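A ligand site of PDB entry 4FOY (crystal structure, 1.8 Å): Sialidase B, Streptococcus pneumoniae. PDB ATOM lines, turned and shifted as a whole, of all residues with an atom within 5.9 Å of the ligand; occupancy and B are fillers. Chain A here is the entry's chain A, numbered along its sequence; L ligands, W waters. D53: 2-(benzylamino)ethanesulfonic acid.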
ATOM      1  N   ARG A 245      -2.795  19.925 -16.467  1.00  0.00           N
ATOM      2  CA  ARG A 245      -4.121  20.106 -17.068  1.00  0.00           C
ATOM      3  C   ARG A 245      -4.107  19.539 -18.485  1.00  0.00           C
ATOM      4  O   ARG A 245      -3.046  19.285 -19.038  1.00  0.00           O
ATOM      5  CB  ARG A 245      -4.518  21.594 -17.120  1.00  0.00           C
ATOM      6  CG  ARG A 245      -5.109  22.152 -15.792  1.00  0.00           C
ATOM      7  CD  ARG A 245      -6.101  23.307 -16.055  1.00  0.00           C
ATOM      8  NE  ARG A 245      -7.187  22.887 -16.940  1.00  0.00           N
ATOM      9  CZ  ARG A 245      -8.024  23.734 -17.549  1.00  0.00           C
ATOM     10  NH1 ARG A 245      -7.899  25.045 -17.338  1.00  0.00           N
ATOM     11  NH2 ARG A 245      -8.969  23.263 -18.353  1.00  0.00           N
ATOM     12  N   ILE A 246      -5.301  19.392 -19.062  1.00  0.00           N
ATOM     13  CA  ILE A 246      -5.447  19.044 -20.485  1.00  0.00           C
ATOM     14  C   ILE A 246      -4.877  17.657 -20.815  1.00  0.00           C
ATOM     15  O   ILE A 246      -3.920  17.541 -21.586  1.00  0.00           O
ATOM     16  CB  ILE A 246      -4.805  20.120 -21.434  1.00  0.00           C
ATOM     17  CG1 ILE A 246      -4.917  21.541 -20.854  1.00  0.00           C
ATOM     18  CG2 ILE A 246      -5.477  20.085 -22.794  1.00  0.00           C
ATOM     19  CD1 ILE A 246      -6.378  22.062 -20.631  1.00  0.00           C
ATOM     20  N   ARG A 264       2.147  21.925 -16.060  1.00  0.00           N
ATOM     21  CA  ARG A 264       2.000  23.354 -15.771  1.00  0.00           C
ATOM     22  C   ARG A 264       2.752  23.750 -14.503  1.00  0.00           C
ATOM     23  O   ARG A 264       2.473  23.250 -13.410  1.00  0.00           O
ATOM     24  CB  ARG A 264       0.519  23.749 -15.691  1.00  0.00           C
ATOM     25  CG  ARG A 264      -0.246  23.461 -17.007  1.00  0.00           C
ATOM     26  CD  ARG A 264      -1.591  24.194 -17.036  1.00  0.00           C
ATOM     27  NE  ARG A 264      -2.223  24.124 -18.358  1.00  0.00           N
ATOM     28  CZ  ARG A 264      -3.301  24.811 -18.717  1.00  0.00           C
ATOM     29  NH1 ARG A 264      -3.896  25.629 -17.852  1.00  0.00           N
ATOM     30  NH2 ARG A 264      -3.780  24.694 -19.950  1.00  0.00           N
ATOM     31  N   ASP A 270      -3.625  28.955 -17.543  1.00  0.00           N
ATOM     32  CA  ASP A 270      -3.295  28.862 -18.971  1.00  0.00           C
ATOM     33  C   ASP A 270      -2.114  29.787 -19.252  1.00  0.00           C
ATOM     34  O   ASP A 270      -1.803  30.671 -18.458  1.00  0.00           O
ATOM     35  CB  ASP A 270      -4.444  29.385 -19.848  1.00  0.00           C
ATOM     36  CG  ASP A 270      -5.603  28.430 -19.962  1.00  0.00           C
ATOM     37  OD1 ASP A 270      -6.591  28.843 -20.613  1.00  0.00           O
ATOM     38  OD2 ASP A 270      -5.531  27.285 -19.449  1.00  0.00           O
ATOM     39  N   SER A 271      -1.474  29.603 -20.410  1.00  0.00           N
ATOM     40  CA  SER A 271      -0.495  30.592 -20.910  1.00  0.00           C
ATOM     41  C   SER A 271      -1.128  31.995 -20.874  1.00  0.00           C
ATOM     42  O   SER A 271      -2.338  32.113 -21.064  1.00  0.00           O
ATOM     43  CB  SER A 271      -0.099  30.235 -22.341  1.00  0.00           C
ATOM     44  OG  SER A 271       0.397  28.896 -22.405  1.00  0.00           O
ATOM     45  N   ILE A 326       0.911  24.500 -24.982  1.00  0.00           N
ATOM     46  CA  ILE A 326      -0.380  24.291 -24.327  1.00  0.00           C
ATOM     47  C   ILE A 326      -1.323  23.593 -25.280  1.00  0.00           C
ATOM     48  O   ILE A 326      -1.247  23.831 -26.478  1.00  0.00           O
ATOM     49  CB  ILE A 326      -0.980  25.654 -23.824  1.00  0.00           C
ATOM     50  CG1 ILE A 326      -2.373  25.476 -23.231  1.00  0.00           C
ATOM     51  CG2 ILE A 326      -0.967  26.723 -24.932  1.00  0.00           C
ATOM     52  CD1 ILE A 326      -2.828  26.695 -22.397  1.00  0.00           C
ATOM     53  N   ASP A 327      -2.183  22.715 -24.750  1.00  0.00           N
ATOM     54  CA  ASP A 327      -3.202  21.993 -25.528  1.00  0.00           C
ATOM     55  C   ASP A 327      -2.613  21.017 -26.563  1.00  0.00           C
ATOM     56  O   ASP A 327      -2.518  21.331 -27.748  1.00  0.00           O
ATOM     57  CB  ASP A 327      -4.148  22.970 -26.239  1.00  0.00           C
ATOM     58  CG  ASP A 327      -5.108  23.660 -25.284  1.00  0.00           C
ATOM     59  OD1 ASP A 327      -5.110  23.310 -24.087  1.00  0.00           O
ATOM     60  OD2 ASP A 327      -5.866  24.554 -25.733  1.00  0.00           O
ATOM     61  N   ASP A 344      -0.148  23.833 -29.134  1.00  0.00           N
ATOM     62  CA  ASP A 344       0.032  25.253 -29.398  1.00  0.00           C
ATOM     63  C   ASP A 344       1.397  25.682 -28.862  1.00  0.00           C
ATOM     64  O   ASP A 344       1.904  25.085 -27.895  1.00  0.00           O
ATOM     65  CB  ASP A 344      -1.043  26.108 -28.697  1.00  0.00           C
ATOM     66  CG  ASP A 344      -2.471  25.778 -29.111  1.00  0.00           C
ATOM     67  OD1 ASP A 344      -2.726  25.303 -30.245  1.00  0.00           O
ATOM     68  OD2 ASP A 344      -3.367  26.037 -28.280  1.00  0.00           O
ATOM     69  N   MET A 346       3.472  29.185 -27.477  1.00  0.00           N
ATOM     70  CA  MET A 346       3.333  30.588 -27.068  1.00  0.00           C
ATOM     71  C   MET A 346       4.719  31.169 -26.784  1.00  0.00           C
ATOM     72  O   MET A 346       5.468  30.620 -25.975  1.00  0.00           O
ATOM     73  CB  MET A 346       2.520  30.675 -25.777  1.00  0.00           C
ATOM     74  CG  MET A 346       1.181  29.973 -25.847  1.00  0.00           C
ATOM     75  SD  MET A 346       0.008  30.941 -26.808  1.00  0.00           S
ATOM     76  CE  MET A 346      -0.831  29.604 -27.656  1.00  0.00           C
ATOM     77  N   GLY A 351      -0.241  34.599 -24.233  1.00  0.00           N
ATOM     78  CA  GLY A 351      -1.375  33.698 -24.046  1.00  0.00           C
ATOM     79  C   GLY A 351      -2.450  34.039 -25.056  1.00  0.00           C
ATOM     80  O   GLY A 351      -2.192  34.832 -25.978  1.00  0.00           O
ATOM     81  N   ASN A 352      -3.642  33.467 -24.924  1.00  0.00           N
ATOM     82  CA  ASN A 352      -4.659  33.694 -25.962  1.00  0.00           C
ATOM     83  C   ASN A 352      -5.254  35.108 -25.935  1.00  0.00           C
ATOM     84  O   ASN A 352      -5.763  35.587 -26.944  1.00  0.00           O
ATOM     85  CB  ASN A 352      -5.747  32.590 -25.975  1.00  0.00           C
ATOM     86  CG  ASN A 352      -6.744  32.698 -24.829  1.00  0.00           C
ATOM     87  OD1 ASN A 352      -6.597  33.504 -23.913  1.00  0.00           O
ATOM     88  ND2 ASN A 352      -7.774  31.850 -24.875  1.00  0.00           N
ATOM     89  N   TYR A 489      -6.311  27.522 -32.908  1.00  0.00           N
ATOM     90  CA  TYR A 489      -5.954  26.871 -31.655  1.00  0.00           C
ATOM     91  C   TYR A 489      -6.249  25.388 -31.751  1.00  0.00           C
ATOM     92  O   TYR A 489      -7.351  24.980 -32.108  1.00  0.00           O
ATOM     93  CB  TYR A 489      -6.734  27.489 -30.497  1.00  0.00           C
ATOM     94  CG  TYR A 489      -6.252  28.882 -30.159  1.00  0.00           C
ATOM     95  CD1 TYR A 489      -5.208  29.085 -29.274  1.00  0.00           C
ATOM     96  CD2 TYR A 489      -6.862  29.999 -30.742  1.00  0.00           C
ATOM     97  CE1 TYR A 489      -4.762  30.364 -28.969  1.00  0.00           C
ATOM     98  CE2 TYR A 489      -6.421  31.287 -30.435  1.00  0.00           C
ATOM     99  CZ  TYR A 489      -5.381  31.454 -29.552  1.00  0.00           C
ATOM    100  OH  TYR A 489      -4.928  32.723 -29.239  1.00  0.00           O
ATOM    101  N   TYR A 509      -9.564  25.357 -33.766  1.00  0.00           N
ATOM    102  CA  TYR A 509     -10.652  26.338 -33.800  1.00  0.00           C
ATOM    103  C   TYR A 509     -10.141  27.773 -33.904  1.00  0.00           C
ATOM    104  O   TYR A 509      -9.005  28.088 -33.524  1.00  0.00           O
ATOM    105  CB  TYR A 509     -11.586  26.196 -32.581  1.00  0.00           C
ATOM    106  CG  TYR A 509     -10.930  26.495 -31.254  1.00  0.00           C
ATOM    107  CD1 TYR A 509     -10.956  27.788 -30.720  1.00  0.00           C
ATOM    108  CD2 TYR A 509     -10.284  25.498 -30.523  1.00  0.00           C
ATOM    109  CE1 TYR A 509     -10.348  28.081 -29.516  1.00  0.00           C
ATOM    110  CE2 TYR A 509      -9.679  25.784 -29.297  1.00  0.00           C
ATOM    111  CZ  TYR A 509      -9.725  27.076 -28.800  1.00  0.00           C
ATOM    112  OH  TYR A 509      -9.121  27.378 -27.594  1.00  0.00           O
ATOM    113  N   THR A 539     -14.598  29.059 -27.629  1.00  0.00           N
ATOM    114  CA  THR A 539     -13.499  28.132 -27.415  1.00  0.00           C
ATOM    115  C   THR A 539     -14.046  26.805 -27.926  1.00  0.00           C
ATOM    116  O   THR A 539     -14.486  25.973 -27.134  1.00  0.00           O
ATOM    117  CB  THR A 539     -13.165  28.053 -25.920  1.00  0.00           C
ATOM    118  OG1 THR A 539     -12.899  29.369 -25.435  1.00  0.00           O
ATOM    119  CG2 THR A 539     -11.966  27.154 -25.658  1.00  0.00           C
ATOM    120  N   GLU A 541     -13.591  23.746 -28.756  1.00  0.00           N
ATOM    121  CA  GLU A 541     -12.780  22.524 -28.689  1.00  0.00           C
ATOM    122  C   GLU A 541     -13.594  21.368 -29.233  1.00  0.00           C
ATOM    123  O   GLU A 541     -14.692  21.065 -28.736  1.00  0.00           O
ATOM    124  CB  GLU A 541     -12.328  22.299 -27.242  1.00  0.00           C
ATOM    125  CG  GLU A 541     -11.343  23.376 -26.764  1.00  0.00           C
ATOM    126  CD  GLU A 541     -11.333  23.542 -25.258  1.00  0.00           C
ATOM    127  OE1 GLU A 541     -10.307  24.021 -24.695  1.00  0.00           O
ATOM    128  OE2 GLU A 541     -12.351  23.169 -24.633  1.00  0.00           O
ATOM    129  N   ARG A 557     -17.438  22.013 -28.151  1.00  0.00           N
ATOM    130  CA  ARG A 557     -17.834  22.930 -27.082  1.00  0.00           C
ATOM    131  C   ARG A 557     -18.344  24.209 -27.697  1.00  0.00           C
ATOM    132  O   ARG A 557     -17.795  24.686 -28.691  1.00  0.00           O
ATOM    133  CB  ARG A 557     -16.587  23.219 -26.224  1.00  0.00           C
ATOM    134  CG  ARG A 557     -16.725  24.317 -25.168  1.00  0.00           C
ATOM    135  CD  ARG A 557     -15.377  24.489 -24.465  1.00  0.00           C
ATOM    136  NE  ARG A 557     -15.336  25.669 -23.607  1.00  0.00           N
ATOM    137  CZ  ARG A 557     -14.283  26.004 -22.868  1.00  0.00           C
ATOM    138  NH1 ARG A 557     -13.194  25.231 -22.886  1.00  0.00           N
ATOM    139  NH2 ARG A 557     -14.313  27.080 -22.115  1.00  0.00           N
ATOM    140  N   TYR A 589     -20.020  28.830 -20.555  1.00  0.00           N
ATOM    141  CA  TYR A 589     -18.645  28.901 -21.081  1.00  0.00           C
ATOM    142  C   TYR A 589     -18.149  27.593 -21.695  1.00  0.00           C
ATOM    143  O   TYR A 589     -17.260  27.602 -22.560  1.00  0.00           O
ATOM    144  CB  TYR A 589     -17.663  29.393 -20.003  1.00  0.00           C
ATOM    145  CG  TYR A 589     -17.765  28.666 -18.691  1.00  0.00           C
ATOM    146  CD1 TYR A 589     -17.051  27.493 -18.466  1.00  0.00           C
ATOM    147  CD2 TYR A 589     -18.570  29.153 -17.664  1.00  0.00           C
ATOM    148  CE1 TYR A 589     -17.140  26.822 -17.266  1.00  0.00           C
ATOM    149  CE2 TYR A 589     -18.672  28.486 -16.460  1.00  0.00           C
ATOM    150  CZ  TYR A 589     -17.939  27.330 -16.260  1.00  0.00           C
ATOM    151  OH  TYR A 589     -18.032  26.668 -15.058  1.00  0.00           O
ATOM    152  N   GLY A 590     -18.730  26.477 -21.257  1.00  0.00           N
ATOM    153  CA  GLY A 590     -18.471  25.181 -21.856  1.00  0.00           C
ATOM    154  C   GLY A 590     -17.241  24.453 -21.336  1.00  0.00           C
ATOM    155  O   GLY A 590     -16.443  25.013 -20.596  1.00  0.00           O
ATOM    156  N   ARG A 619     -18.176  22.885 -13.601  1.00  0.00           N
ATOM    157  CA  ARG A 619     -17.524  21.721 -14.203  1.00  0.00           C
ATOM    158  C   ARG A 619     -17.560  20.601 -13.168  1.00  0.00           C
ATOM    159  O   ARG A 619     -16.630  20.433 -12.371  1.00  0.00           O
ATOM    160  CB  ARG A 619     -16.106  22.074 -14.661  1.00  0.00           C
ATOM    161  CG  ARG A 619     -16.108  23.082 -15.832  1.00  0.00           C
ATOM    162  CD  ARG A 619     -14.700  23.366 -16.356  1.00  0.00           C
ATOM    163  NE  ARG A 619     -14.713  24.003 -17.677  1.00  0.00           N
ATOM    164  CZ  ARG A 619     -13.666  24.624 -18.222  1.00  0.00           C
ATOM    165  NH1 ARG A 619     -12.519  24.703 -17.556  1.00  0.00           N
ATOM    166  NH2 ARG A 619     -13.769  25.176 -19.432  1.00  0.00           N
ATOM    167  N   TYR A 653     -11.891  18.861 -18.056  1.00  0.00           N
ATOM    168  CA  TYR A 653     -11.376  18.317 -19.319  1.00  0.00           C
ATOM    169  C   TYR A 653     -11.126  16.827 -19.142  1.00  0.00           C
ATOM    170  O   TYR A 653     -10.863  16.369 -18.030  1.00  0.00           O
ATOM    171  CB  TYR A 653     -10.067  18.983 -19.735  1.00  0.00           C
ATOM    172  CG  TYR A 653     -10.237  20.338 -20.418  1.00  0.00           C
ATOM    173  CD1 TYR A 653     -11.150  21.273 -19.943  1.00  0.00           C
ATOM    174  CD2 TYR A 653      -9.474  20.663 -21.518  1.00  0.00           C
ATOM    175  CE1 TYR A 653     -11.288  22.513 -20.562  1.00  0.00           C
ATOM    176  CE2 TYR A 653      -9.602  21.901 -22.152  1.00  0.00           C
ATOM    177  CZ  TYR A 653     -10.505  22.824 -21.659  1.00  0.00           C
ATOM    178  OH  TYR A 653     -10.637  24.049 -22.293  1.00  0.00           O
ATOM    179  N   SER A 673     -11.971  23.149 -13.138  1.00  0.00           N
ATOM    180  CA  SER A 673     -10.846  23.917 -13.649  1.00  0.00           C
ATOM    181  C   SER A 673     -11.251  25.296 -14.169  1.00  0.00           C
ATOM    182  O   SER A 673     -10.413  26.018 -14.719  1.00  0.00           O
ATOM    183  CB  SER A 673     -10.070  23.114 -14.719  1.00  0.00           C
ATOM    184  OG  SER A 673     -10.893  22.766 -15.817  1.00  0.00           O
ATOM    185  N   TRP A 674     -12.515  25.676 -13.995  1.00  0.00           N
ATOM    186  CA  TRP A 674     -12.966  27.029 -14.317  1.00  0.00           C
ATOM    187  C   TRP A 674     -12.987  27.881 -13.047  1.00  0.00           C
ATOM    188  O   TRP A 674     -12.557  29.044 -13.052  1.00  0.00           O
ATOM    189  CB  TRP A 674     -14.370  27.006 -14.948  1.00  0.00           C
ATOM    190  CG  TRP A 674     -14.825  28.371 -15.466  1.00  0.00           C
ATOM    191  CD1 TRP A 674     -15.621  29.274 -14.808  1.00  0.00           C
ATOM    192  CD2 TRP A 674     -14.507  28.958 -16.739  1.00  0.00           C
ATOM    193  NE1 TRP A 674     -15.821  30.388 -15.600  1.00  0.00           N
ATOM    194  CE2 TRP A 674     -15.147  30.217 -16.788  1.00  0.00           C
ATOM    195  CE3 TRP A 674     -13.748  28.545 -17.839  1.00  0.00           C
ATOM    196  CZ2 TRP A 674     -15.051  31.054 -17.900  1.00  0.00           C
ATOM    197  CZ3 TRP A 674     -13.660  29.377 -18.949  1.00  0.00           C
ATOM    198  CH2 TRP A 674     -14.297  30.620 -18.969  1.00  0.00           C
HETATM  199  CAD D53 L   1      -3.468  29.266 -25.237  1.00  0.00           C
HETATM  200  CAE D53 L   1      -4.163  28.230 -25.886  1.00  0.00           C
HETATM  201  CAF D53 L   1      -4.060  29.969 -24.176  1.00  0.00           C
HETATM  202  CAG D53 L   1      -5.458  27.907 -25.481  1.00  0.00           C
HETATM  203  CAH D53 L   1      -5.355  29.646 -23.771  1.00  0.00           C
HETATM  204  CAI D53 L   1      -8.872  27.275 -22.310  1.00  0.00           C
HETATM  205  CAJ D53 L   1      -9.012  26.486 -21.014  1.00  0.00           C
HETATM  206  CAK D53 L   1      -7.470  28.272 -23.982  1.00  0.00           C
HETATM  207  CAM D53 L   1      -6.067  28.630 -24.445  1.00  0.00           C
HETATM  208  NAL D53 L   1      -7.490  27.389 -22.802  1.00  0.00           N
HETATM  209  OAA D53 L   1     -10.368  25.947 -18.766  1.00  0.00           O
HETATM  210  OAB D53 L   1     -10.270  28.262 -19.481  1.00  0.00           O
HETATM  211  OAC D53 L   1     -11.689  26.678 -20.670  1.00  0.00           O
HETATM  212  SAN D53 L   1     -10.422  26.875 -19.953  1.00  0.00           S
HETATM  213  O   HOH W   1      -6.398  25.101 -22.346  1.00  0.00           O
HETATM  214  O   HOH W   2      -8.064  28.464 -17.806  1.00  0.00           O
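Water W1 lies within hydrogen-bond range of NAL of the ligand and OD1 of Asp 327.
Water W2 lies within hydrogen-bond range of an oxygen (OAB) of the ligand, the side-chain carboxylate (OD1) of Asp 270 and the guanidinium group (NH1) of Arg 245.
NH1 of Arg 619 lies within salt-bridge range of OAA of the ligand, 2.8 Å away.
A nitrogen (NAL) of the ligand lies within salt-bridge range of the side-chain carboxylate (OD1) of Asp 270.
NH1 of Arg 245 lies within salt-bridge range of OAA of the ligand (3.0 Å).
An oxygen (OAC) of the ligand lies within salt-bridge range of the guanidinium group (NH2) of Arg 557, 3.0 Å away.
An oxygen (OAC) of the ligand lies close to the side-chain hydroxyl (OH) of Tyr 653 (3.3 Å).
NH2 of Arg 619 sits at hydrogen-bond distance from O of Gly 590 (2.9 Å).
The side-chain carboxylate (OD2) of Asp 270 lies within salt-bridge range of the guanidinium group (NH1) of Arg 264 (2.8 Å).
The guanidinium group (NH2) of Arg 245 lies within hydrogen-bond range of the side-chain hydroxyl (OG) of Ser 673 (3.2 Å).
NH1 of Arg 557 sits at hydrogen-bond distance from OH of Tyr 653, at 2.9 Å.
NE of Arg 557 lies close to O of Gly 590, at 3.3 Å.
OE1 of Glu 541 is in hydrogen-bond range of OH of Tyr 653 (2.4 Å).
The backbone carbonyl oxygen (O) of Ile 326 sits at hydrogen-bond distance from the backbone NH (N) of Asp 344.
The backbone carbonyl oxygen (O) of Tyr 489 lies within hydrogen-bond range of the backbone NH (N) of Tyr 509, at 2.8 Å.
Residues that only touch the ligand: Asp 344 (3.3 Å), Asp 327 (3.4 Å), Asn 352 (3.5 Å), Ile 326 (3.6 Å), Met 346 (3.6 Å), Trp 674 (3.6 Å) and Tyr 489 (3.6 Å).
Within 4 Å of the ligand: Arg 245, Asp 270, Ile 326, Asp 327, Asp 344, Met 346, Asn 352, Tyr 489, Arg 557, Arg 619, Tyr 653 and Trp 674.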
